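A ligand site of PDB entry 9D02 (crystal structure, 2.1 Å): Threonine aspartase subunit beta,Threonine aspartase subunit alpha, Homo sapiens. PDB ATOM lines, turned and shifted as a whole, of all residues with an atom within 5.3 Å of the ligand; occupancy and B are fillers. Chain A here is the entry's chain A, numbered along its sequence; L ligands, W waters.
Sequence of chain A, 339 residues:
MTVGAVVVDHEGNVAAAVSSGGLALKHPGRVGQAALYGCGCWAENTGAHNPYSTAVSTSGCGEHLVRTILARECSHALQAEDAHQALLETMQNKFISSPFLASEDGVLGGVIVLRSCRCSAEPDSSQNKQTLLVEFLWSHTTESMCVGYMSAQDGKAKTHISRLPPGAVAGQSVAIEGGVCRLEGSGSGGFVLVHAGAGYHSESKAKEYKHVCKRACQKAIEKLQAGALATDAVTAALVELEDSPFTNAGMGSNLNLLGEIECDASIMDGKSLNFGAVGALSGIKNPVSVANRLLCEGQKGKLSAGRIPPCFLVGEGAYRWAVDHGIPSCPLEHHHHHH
A carbon (C14) of the ligand is bonded to the side-chain sulfur (SG) of Cys 61.
An oxygen (O2) of the ligand lies within hydrogen-bond range of the backbone NH (N) of Cys 61 (3.4 Å).
The side-chain amide nitrogen of Asn 248 is in hydrogen-bond range of an oxygen (O3) of the ligand, 2.7 Å away.
N of Thr 2 sits at hydrogen-bond distance from O3 of the ligand.
The side-chain amide oxygen (OD1) of Asn 248 lies within hydrogen-bond range of the backbone NH (N) of Asn 254 (2.8 Å).
ND2 of Asn 248 lies within hydrogen-bond range of O of Gly 22 (2.9 Å).
O of Ser 144 sits at hydrogen-bond distance from N of Gly 199 (2.9 Å).
The side-chain hydroxyl (OH) of Tyr 209 is in hydrogen-bond range of the backbone carbonyl oxygen (O) of Phe 246 (2.9 Å).
The backbone carbonyl oxygen (O) of Gly 60 sits at hydrogen-bond distance from the side-chain hydroxyl (OG1) of Thr 2 (2.9 Å).
O of Gly 22 is in hydrogen-bond range of ND2 of Asn 254 (3.2 Å).
O of Tyr 209 lies close to SG of Cys 146 (3.8 Å).
The side-chain hydroxyl (OG1) of Thr 2 is in hydrogen-bond range of the side-chain hydroxyl (OG) of Ser 20, 2.9 Å away.
An oxygen (O2) of the ligand lies close to the backbone carbonyl oxygen (O) of Gly 60 (3.5 Å).
O of Gly 197 lies close to F1 of the ligand (3.2 Å).
The backbone NH (N) of Ser 202 lies close to a fluorine (F4) of the ligand (3.4 Å).
CB of Ser 144 touches F4 of the ligand, 3.6 Å away.
CB of Cys 146 touches F1 of the ligand (3.1 Å).
Ile 161 touches the ligand (CD1 to F2, 3.2 Å).
Ala 196 touches the ligand (O to C2, 3.5 Å).
O of Ala 198 touches C6 of the ligand, 3.1 Å away.
Tyr 200 touches the ligand (O to C16, 3.2 Å).
CA of His 201 touches F4 of the ligand (3.6 Å).
Tyr 209 touches the ligand.
Phe 246 touches the ligand.
C of Thr 247 touches C12 of the ligand (3.2 Å).
O of Gly 252 touches C12 of the ligand, 3.7 Å away.
OD1 of Asn 254 touches C10 of the ligand, 3.7 Å away.
Of the 28 residues printed, 18 come within 4 Å of the ligand.
The nearest printed residue that does not touch the ligand is Pro 245 (4.05 Å).
Water W1 lies within hydrogen-bond range of the backbone NH (N) of Gly 60 (2.8 Å), an oxygen (O2) of the ligand (2.8 Å), the backbone carbonyl oxygen (O) of Thr 2 (3.0 Å) and the backbone NH (N) of Ala 198 (3.0 Å).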
ATOM      1  N   THR A   2      23.118 -20.656   3.836  1.00  0.00           N
ATOM      2  CA  THR A   2      22.418 -19.384   3.722  1.00  0.00           C
ATOM      3  C   THR A   2      23.144 -18.519   2.725  1.00  0.00           C
ATOM      4  O   THR A   2      24.385 -18.381   2.774  1.00  0.00           O
ATOM      5  CB  THR A   2      22.330 -18.683   5.093  1.00  0.00           C
ATOM      6  OG1 THR A   2      21.723 -19.572   6.026  1.00  0.00           O
ATOM      7  CG2 THR A   2      21.498 -17.404   5.031  1.00  0.00           C
ATOM      8  N   SER A  20      17.755 -19.918   2.623  1.00  0.00           N
ATOM      9  CA  SER A  20      18.513 -20.875   3.418  1.00  0.00           C
ATOM     10  C   SER A  20      17.812 -22.218   3.450  1.00  0.00           C
ATOM     11  O   SER A  20      16.591 -22.303   3.296  1.00  0.00           O
ATOM     12  CB  SER A  20      18.708 -20.408   4.856  1.00  0.00           C
ATOM     13  OG  SER A  20      19.472 -21.399   5.573  1.00  0.00           O
ATOM     14  N   GLY A  22      18.506 -23.993   6.313  1.00  0.00           N
ATOM     15  CA  GLY A  22      18.386 -24.205   7.740  1.00  0.00           C
ATOM     16  C   GLY A  22      19.384 -25.243   8.227  1.00  0.00           C
ATOM     17  O   GLY A  22      20.239 -25.735   7.492  1.00  0.00           O
ATOM     18  N   LEU A  23      19.245 -25.586   9.498  1.00  0.00           N
ATOM     19  CA  LEU A  23      20.169 -26.512  10.152  1.00  0.00           C
ATOM     20  C   LEU A  23      20.003 -27.916   9.590  1.00  0.00           C
ATOM     21  O   LEU A  23      18.889 -28.362   9.313  1.00  0.00           O
ATOM     22  CB  LEU A  23      19.931 -26.513  11.665  1.00  0.00           C
ATOM     23  CG  LEU A  23      20.353 -25.244  12.412  1.00  0.00           C
ATOM     24  CD1 LEU A  23      19.690 -25.227  13.775  1.00  0.00           C
ATOM     25  CD2 LEU A  23      21.871 -25.182  12.583  1.00  0.00           C
ATOM     26  N   SER A  59      24.062 -13.955   7.025  1.00  0.00           N
ATOM     27  CA  SER A  59      24.710 -15.217   6.704  1.00  0.00           C
ATOM     28  C   SER A  59      24.836 -16.012   7.999  1.00  0.00           C
ATOM     29  O   SER A  59      24.678 -15.480   9.104  1.00  0.00           O
ATOM     30  CB  SER A  59      26.084 -14.999   6.054  1.00  0.00           C
ATOM     31  OG  SER A  59      26.946 -14.210   6.867  1.00  0.00           O
ATOM     32  N   GLY A  60      25.184 -17.291   7.859  1.00  0.00           N
ATOM     33  CA  GLY A  60      25.135 -18.199   8.983  1.00  0.00           C
ATOM     34  C   GLY A  60      23.721 -18.717   9.181  1.00  0.00           C
ATOM     35  O   GLY A  60      22.799 -18.363   8.452  1.00  0.00           O
ATOM     36  N   CYS A  61      23.549 -19.584  10.179  1.00  0.00           N
ATOM     37  CA  CYS A  61      22.203 -20.071  10.472  1.00  0.00           C
ATOM     38  C   CYS A  61      22.074 -20.295  11.970  1.00  0.00           C
ATOM     39  O   CYS A  61      22.927 -19.869  12.757  1.00  0.00           O
ATOM     40  CB  CYS A  61      21.868 -21.326   9.640  1.00  0.00           C
ATOM     41  SG  CYS A  61      22.929 -22.759   9.893  1.00  0.00           S
ATOM     42  N   GLY A  62      20.974 -20.914  12.373  1.00  0.00           N
ATOM     43  CA  GLY A  62      20.695 -21.122  13.774  1.00  0.00           C
ATOM     44  C   GLY A  62      19.823 -20.013  14.329  1.00  0.00           C
ATOM     45  O   GLY A  62      19.196 -19.235  13.602  1.00  0.00           O
ATOM     46  N   SER A 144      35.105 -17.931   7.782  1.00  0.00           N
ATOM     47  CA  SER A 144      35.168 -17.427   6.415  1.00  0.00           C
ATOM     48  C   SER A 144      33.785 -16.990   5.955  1.00  0.00           C
ATOM     49  O   SER A 144      32.759 -17.371   6.526  1.00  0.00           O
ATOM     50  CB  SER A 144      35.712 -18.468   5.440  1.00  0.00           C
ATOM     51  OG  SER A 144      37.063 -18.779   5.704  1.00  0.00           O
ATOM     52  N   MET A 145      33.796 -16.205   4.878  1.00  0.00           N
ATOM     53  CA  MET A 145      32.600 -15.754   4.201  1.00  0.00           C
ATOM     54  C   MET A 145      33.014 -15.405   2.785  1.00  0.00           C
ATOM     55  O   MET A 145      34.093 -14.832   2.588  1.00  0.00           O
ATOM     56  CB  MET A 145      31.959 -14.565   4.933  1.00  0.00           C
ATOM     57  CG  MET A 145      30.648 -14.053   4.337  1.00  0.00           C
ATOM     58  SD  MET A 145      29.989 -12.732   5.361  1.00  0.00           S
ATOM     59  CE  MET A 145      28.563 -12.189   4.448  1.00  0.00           C
ATOM     60  N   CYS A 146      32.208 -15.807   1.810  1.00  0.00           N
ATOM     61  CA  CYS A 146      32.488 -15.513   0.411  1.00  0.00           C
ATOM     62  C   CYS A 146      31.517 -14.473  -0.111  1.00  0.00           C
ATOM     63  O   CYS A 146      30.291 -14.688  -0.087  1.00  0.00           O
ATOM     64  CB  CYS A 146      32.421 -16.783  -0.432  1.00  0.00           C
ATOM     65  SG  CYS A 146      32.951 -16.504  -2.154  1.00  0.00           S
ATOM     66  N   ILE A 161      37.099 -13.849  -0.689  1.00  0.00           N
ATOM     67  CA  ILE A 161      36.878 -14.739   0.445  1.00  0.00           C
ATOM     68  C   ILE A 161      37.424 -14.037   1.680  1.00  0.00           C
ATOM     69  O   ILE A 161      38.644 -13.828   1.810  1.00  0.00           O
ATOM     70  CB  ILE A 161      37.527 -16.104   0.207  1.00  0.00           C
ATOM     71  CG1 ILE A 161      36.645 -16.907  -0.765  1.00  0.00           C
ATOM     72  CG2 ILE A 161      37.749 -16.851   1.529  1.00  0.00           C
ATOM     73  CD1 ILE A 161      37.004 -18.347  -0.865  1.00  0.00           C
ATOM     74  N   ALA A 196      27.747 -16.120  -0.647  1.00  0.00           N
ATOM     75  CA  ALA A 196      27.404 -17.521  -0.848  1.00  0.00           C
ATOM     76  C   ALA A 196      27.393 -18.322   0.438  1.00  0.00           C
ATOM     77  O   ALA A 196      27.190 -19.538   0.394  1.00  0.00           O
ATOM     78  CB  ALA A 196      28.384 -18.156  -1.839  1.00  0.00           C
ATOM     79  N   GLY A 197      27.603 -17.689   1.574  1.00  0.00           N
ATOM     80  CA  GLY A 197      27.564 -18.361   2.860  1.00  0.00           C
ATOM     81  C   GLY A 197      28.704 -17.881   3.748  1.00  0.00           C
ATOM     82  O   GLY A 197      29.741 -17.404   3.273  1.00  0.00           O
ATOM     83  N   ALA A 198      28.499 -18.014   5.065  1.00  0.00           N
ATOM     84  CA  ALA A 198      29.545 -17.733   6.044  1.00  0.00           C
ATOM     85  C   ALA A 198      29.655 -18.934   6.966  1.00  0.00           C
ATOM     86  O   ALA A 198      28.670 -19.333   7.589  1.00  0.00           O
ATOM     87  CB  ALA A 198      29.239 -16.468   6.855  1.00  0.00           C
ATOM     88  N   GLY A 199      30.856 -19.527   7.030  1.00  0.00           N
ATOM     89  CA  GLY A 199      31.078 -20.709   7.841  1.00  0.00           C
ATOM     90  C   GLY A 199      32.524 -21.159   7.873  1.00  0.00           C
ATOM     91  O   GLY A 199      33.453 -20.352   7.886  1.00  0.00           O
ATOM     92  N   TYR A 200      32.716 -22.482   7.908  1.00  0.00           N
ATOM     93  CA  TYR A 200      34.053 -23.044   7.938  1.00  0.00           C
ATOM     94  C   TYR A 200      34.750 -22.797   6.607  1.00  0.00           C
ATOM     95  O   TYR A 200      34.104 -22.805   5.545  1.00  0.00           O
ATOM     96  CB  TYR A 200      33.978 -24.547   8.200  1.00  0.00           C
ATOM     97  CG  TYR A 200      33.487 -24.930   9.571  1.00  0.00           C
ATOM     98  CD1 TYR A 200      34.229 -24.639  10.708  1.00  0.00           C
ATOM     99  CD2 TYR A 200      32.279 -25.599   9.728  1.00  0.00           C
ATOM    100  CE1 TYR A 200      33.793 -24.992  11.965  1.00  0.00           C
ATOM    101  CE2 TYR A 200      31.824 -25.959  10.982  1.00  0.00           C
ATOM    102  CZ  TYR A 200      32.585 -25.654  12.101  1.00  0.00           C
ATOM    103  OH  TYR A 200      32.145 -26.020  13.348  1.00  0.00           O
ATOM    104  N   HIS A 201      36.063 -22.560   6.652  1.00  0.00           N
ATOM    105  CA  HIS A 201      36.812 -22.385   5.422  1.00  0.00           C
ATOM    106  C   HIS A 201      36.898 -23.695   4.660  1.00  0.00           C
ATOM    107  O   HIS A 201      37.031 -24.766   5.253  1.00  0.00           O
ATOM    108  CB  HIS A 201      38.227 -21.852   5.717  1.00  0.00           C
ATOM    109  CG  HIS A 201      38.983 -21.438   4.485  1.00  0.00           C
ATOM    110  ND1 HIS A 201      38.576 -20.380   3.697  1.00  0.00           N
ATOM    111  CD2 HIS A 201      40.097 -21.942   3.902  1.00  0.00           C
ATOM    112  CE1 HIS A 201      39.422 -20.250   2.679  1.00  0.00           C
ATOM    113  NE2 HIS A 201      40.345 -21.189   2.788  1.00  0.00           N
ATOM    114  N   SER A 202      36.831 -23.614   3.338  1.00  0.00           N
ATOM    115  CA  SER A 202      36.989 -24.779   2.474  1.00  0.00           C
ATOM    116  C   SER A 202      37.891 -24.355   1.315  1.00  0.00           C
ATOM    117  O   SER A 202      37.444 -23.629   0.428  1.00  0.00           O
ATOM    118  CB  SER A 202      35.635 -25.284   1.973  1.00  0.00           C
ATOM    119  OG  SER A 202      35.755 -26.565   1.370  1.00  0.00           O
ATOM    120  N   LYS A 205      36.352 -26.021  -3.466  1.00  0.00           N
ATOM    121  CA  LYS A 205      35.049 -25.373  -3.620  1.00  0.00           C
ATOM    122  C   LYS A 205      35.086 -23.877  -3.313  1.00  0.00           C
ATOM    123  O   LYS A 205      34.102 -23.166  -3.557  1.00  0.00           O
ATOM    124  CB  LYS A 205      33.977 -26.060  -2.761  1.00  0.00           C
ATOM    125  N   ALA A 206      36.220 -23.362  -2.812  1.00  0.00           N
ATOM    126  CA  ALA A 206      36.375 -21.920  -2.678  1.00  0.00           C
ATOM    127  C   ALA A 206      36.204 -21.213  -4.016  1.00  0.00           C
ATOM    128  O   ALA A 206      35.546 -20.179  -4.106  1.00  0.00           O
ATOM    129  CB  ALA A 206      37.733 -21.588  -2.076  1.00  0.00           C
ATOM    130  N   TYR A 209      32.447 -21.196  -4.926  1.00  0.00           N
ATOM    131  CA  TYR A 209      31.695 -20.158  -4.224  1.00  0.00           C
ATOM    132  C   TYR A 209      31.931 -18.792  -4.837  1.00  0.00           C
ATOM    133  O   TYR A 209      30.988 -18.023  -5.016  1.00  0.00           O
ATOM    134  CB  TYR A 209      32.098 -20.139  -2.755  1.00  0.00           C
ATOM    135  CG  TYR A 209      31.544 -21.280  -1.948  1.00  0.00           C
ATOM    136  CD1 TYR A 209      30.186 -21.597  -1.995  1.00  0.00           C
ATOM    137  CD2 TYR A 209      32.368 -22.041  -1.148  1.00  0.00           C
ATOM    138  CE1 TYR A 209      29.684 -22.644  -1.248  1.00  0.00           C
ATOM    139  CE2 TYR A 209      31.878 -23.086  -0.409  1.00  0.00           C
ATOM    140  CZ  TYR A 209      30.537 -23.388  -0.464  1.00  0.00           C
ATOM    141  OH  TYR A 209      30.056 -24.429   0.277  1.00  0.00           O
ATOM    142  N   PRO A 245      24.794 -26.194  -6.229  1.00  0.00           N
ATOM    143  CA  PRO A 245      24.682 -27.345  -5.321  1.00  0.00           C
ATOM    144  C   PRO A 245      25.508 -27.196  -4.058  1.00  0.00           C
ATOM    145  O   PRO A 245      25.284 -27.936  -3.095  1.00  0.00           O
ATOM    146  CB  PRO A 245      25.158 -28.518  -6.185  1.00  0.00           C
ATOM    147  CG  PRO A 245      26.026 -27.891  -7.229  1.00  0.00           C
ATOM    148  CD  PRO A 245      25.385 -26.568  -7.530  1.00  0.00           C
ATOM    149  N   PHE A 246      26.457 -26.250  -4.025  1.00  0.00           N
ATOM    150  CA  PHE A 246      27.345 -26.090  -2.883  1.00  0.00           C
ATOM    151  C   PHE A 246      26.792 -25.163  -1.805  1.00  0.00           C
ATOM    152  O   PHE A 246      27.411 -25.056  -0.739  1.00  0.00           O
ATOM    153  CB  PHE A 246      28.717 -25.583  -3.357  1.00  0.00           C
ATOM    154  CG  PHE A 246      29.329 -26.428  -4.451  1.00  0.00           C
ATOM    155  CD1 PHE A 246      29.835 -27.696  -4.175  1.00  0.00           C
ATOM    156  CD2 PHE A 246      29.374 -25.962  -5.756  1.00  0.00           C
ATOM    157  CE1 PHE A 246      30.393 -28.469  -5.185  1.00  0.00           C
ATOM    158  CE2 PHE A 246      29.913 -26.743  -6.770  1.00  0.00           C
ATOM    159  CZ  PHE A 246      30.423 -27.996  -6.484  1.00  0.00           C
ATOM    160  N   THR A 247      25.698 -24.448  -2.053  1.00  0.00           N
ATOM    161  CA  THR A 247      25.129 -23.552  -1.058  1.00  0.00           C
ATOM    162  C   THR A 247      23.955 -24.214  -0.338  1.00  0.00           C
ATOM    163  O   THR A 247      23.164 -24.952  -0.945  1.00  0.00           O
ATOM    164  CB  THR A 247      24.643 -22.231  -1.665  1.00  0.00           C
ATOM    165  OG1 THR A 247      23.602 -22.484  -2.615  1.00  0.00           O
ATOM    166  CG2 THR A 247      25.789 -21.493  -2.327  1.00  0.00           C
ATOM    167  N   ASN A 248      23.842 -23.923   0.956  1.00  0.00           N
ATOM    168  CA  ASN A 248      22.731 -24.428   1.768  1.00  0.00           C
ATOM    169  C   ASN A 248      21.505 -23.534   1.575  1.00  0.00           C
ATOM    170  O   ASN A 248      21.099 -22.777   2.445  1.00  0.00           O
ATOM    171  CB  ASN A 248      23.100 -24.494   3.249  1.00  0.00           C
ATOM    172  CG  ASN A 248      21.930 -25.018   4.069  1.00  0.00           C
ATOM    173  OD1 ASN A 248      21.137 -25.802   3.569  1.00  0.00           O
ATOM    174  ND2 ASN A 248      21.803 -24.579   5.314  1.00  0.00           N
ATOM    175  N   GLY A 252      20.372 -28.497  -3.094  1.00  0.00           N
ATOM    176  CA  GLY A 252      21.465 -28.861  -2.212  1.00  0.00           C
ATOM    177  C   GLY A 252      21.283 -28.436  -0.762  1.00  0.00           C
ATOM    178  O   GLY A 252      22.218 -28.571   0.029  1.00  0.00           O
ATOM    179  N   ASN A 254      20.617 -28.524   3.105  1.00  0.00           N
ATOM    180  CA  ASN A 254      20.684 -29.533   4.161  1.00  0.00           C
ATOM    181  C   ASN A 254      19.369 -30.285   4.303  1.00  0.00           C
ATOM    182  O   ASN A 254      18.288 -29.701   4.195  1.00  0.00           O
ATOM    183  CB  ASN A 254      21.011 -28.846   5.493  1.00  0.00           C
ATOM    184  CG  ASN A 254      22.442 -28.422   5.576  1.00  0.00           C
ATOM    185  OD1 ASN A 254      23.278 -28.960   4.862  1.00  0.00           O
ATOM    186  ND2 ASN A 254      22.741 -27.503   6.466  1.00  0.00           N
HETATM  187  C1  LIG L   1      31.027 -20.172   1.778  1.00  0.00           C
HETATM  188  C2  LIG L   1      29.956 -21.030   1.872  1.00  0.00           C
HETATM  189  C3  LIG L   1      29.987 -22.092   2.761  1.00  0.00           C
HETATM  190  C4  LIG L   1      28.819 -23.045   2.874  1.00  0.00           C
HETATM  191  C5  LIG L   1      28.048 -21.753   4.844  1.00  0.00           C
HETATM  192  C6  LIG L   1      27.519 -21.946   6.270  1.00  0.00           C
HETATM  193  C7  LIG L   1      26.484 -24.161   5.616  1.00  0.00           C
HETATM  194  C8  LIG L   1      26.885 -23.853   4.180  1.00  0.00           C
HETATM  195  C9  LIG L   1      26.937 -25.093   3.279  1.00  0.00           C
HETATM  196  C10 LIG L   1      26.226 -27.407   3.244  1.00  0.00           C
HETATM  197  C11 LIG L   1      25.764 -27.071   1.890  1.00  0.00           C
HETATM  198  C12 LIG L   1      25.378 -26.833   0.799  1.00  0.00           C
HETATM  199  C13 LIG L   1      25.221 -23.250   8.616  1.00  0.00           C
HETATM  200  C14 LIG L   1      24.692 -22.802   9.728  1.00  0.00           C
HETATM  201  C15 LIG L   1      31.122 -22.289   3.542  1.00  0.00           C
HETATM  202  C16 LIG L   1      32.189 -21.422   3.446  1.00  0.00           C
HETATM  203  C17 LIG L   1      32.137 -20.365   2.563  1.00  0.00           C
HETATM  204  C18 LIG L   1      34.438 -19.909   1.932  1.00  0.00           C
HETATM  205  F1  LIG L   1      30.967 -19.127   0.904  1.00  0.00           F
HETATM  206  F2  LIG L   1      35.245 -18.865   1.708  1.00  0.00           F
HETATM  207  F3  LIG L   1      34.316 -20.536   0.774  1.00  0.00           F
HETATM  208  F4  LIG L   1      35.094 -20.748   2.744  1.00  0.00           F
HETATM  209  N1  LIG L   1      28.127 -23.060   4.172  1.00  0.00           N
HETATM  210  N2  LIG L   1      26.322 -22.814   6.192  1.00  0.00           N
HETATM  211  O1  LIG L   1      26.374 -26.198   4.008  1.00  0.00           O
HETATM  212  O2  LIG L   1      24.976 -20.822   7.373  1.00  0.00           O
HETATM  213  O3  LIG L   1      23.660 -22.905   6.271  1.00  0.00           O
HETATM  214  O4  LIG L   1      33.239 -19.490   2.443  1.00  0.00           O
HETATM  215  S1  LIG L   1      24.914 -22.377   7.087  1.00  0.00           S
HETATM  216  O   HOH W   1      25.605 -18.763   5.510  1.00  0.00           O
HETATM  217  O   HOH W   2      29.891 -24.177   5.778  1.00  0.00           O
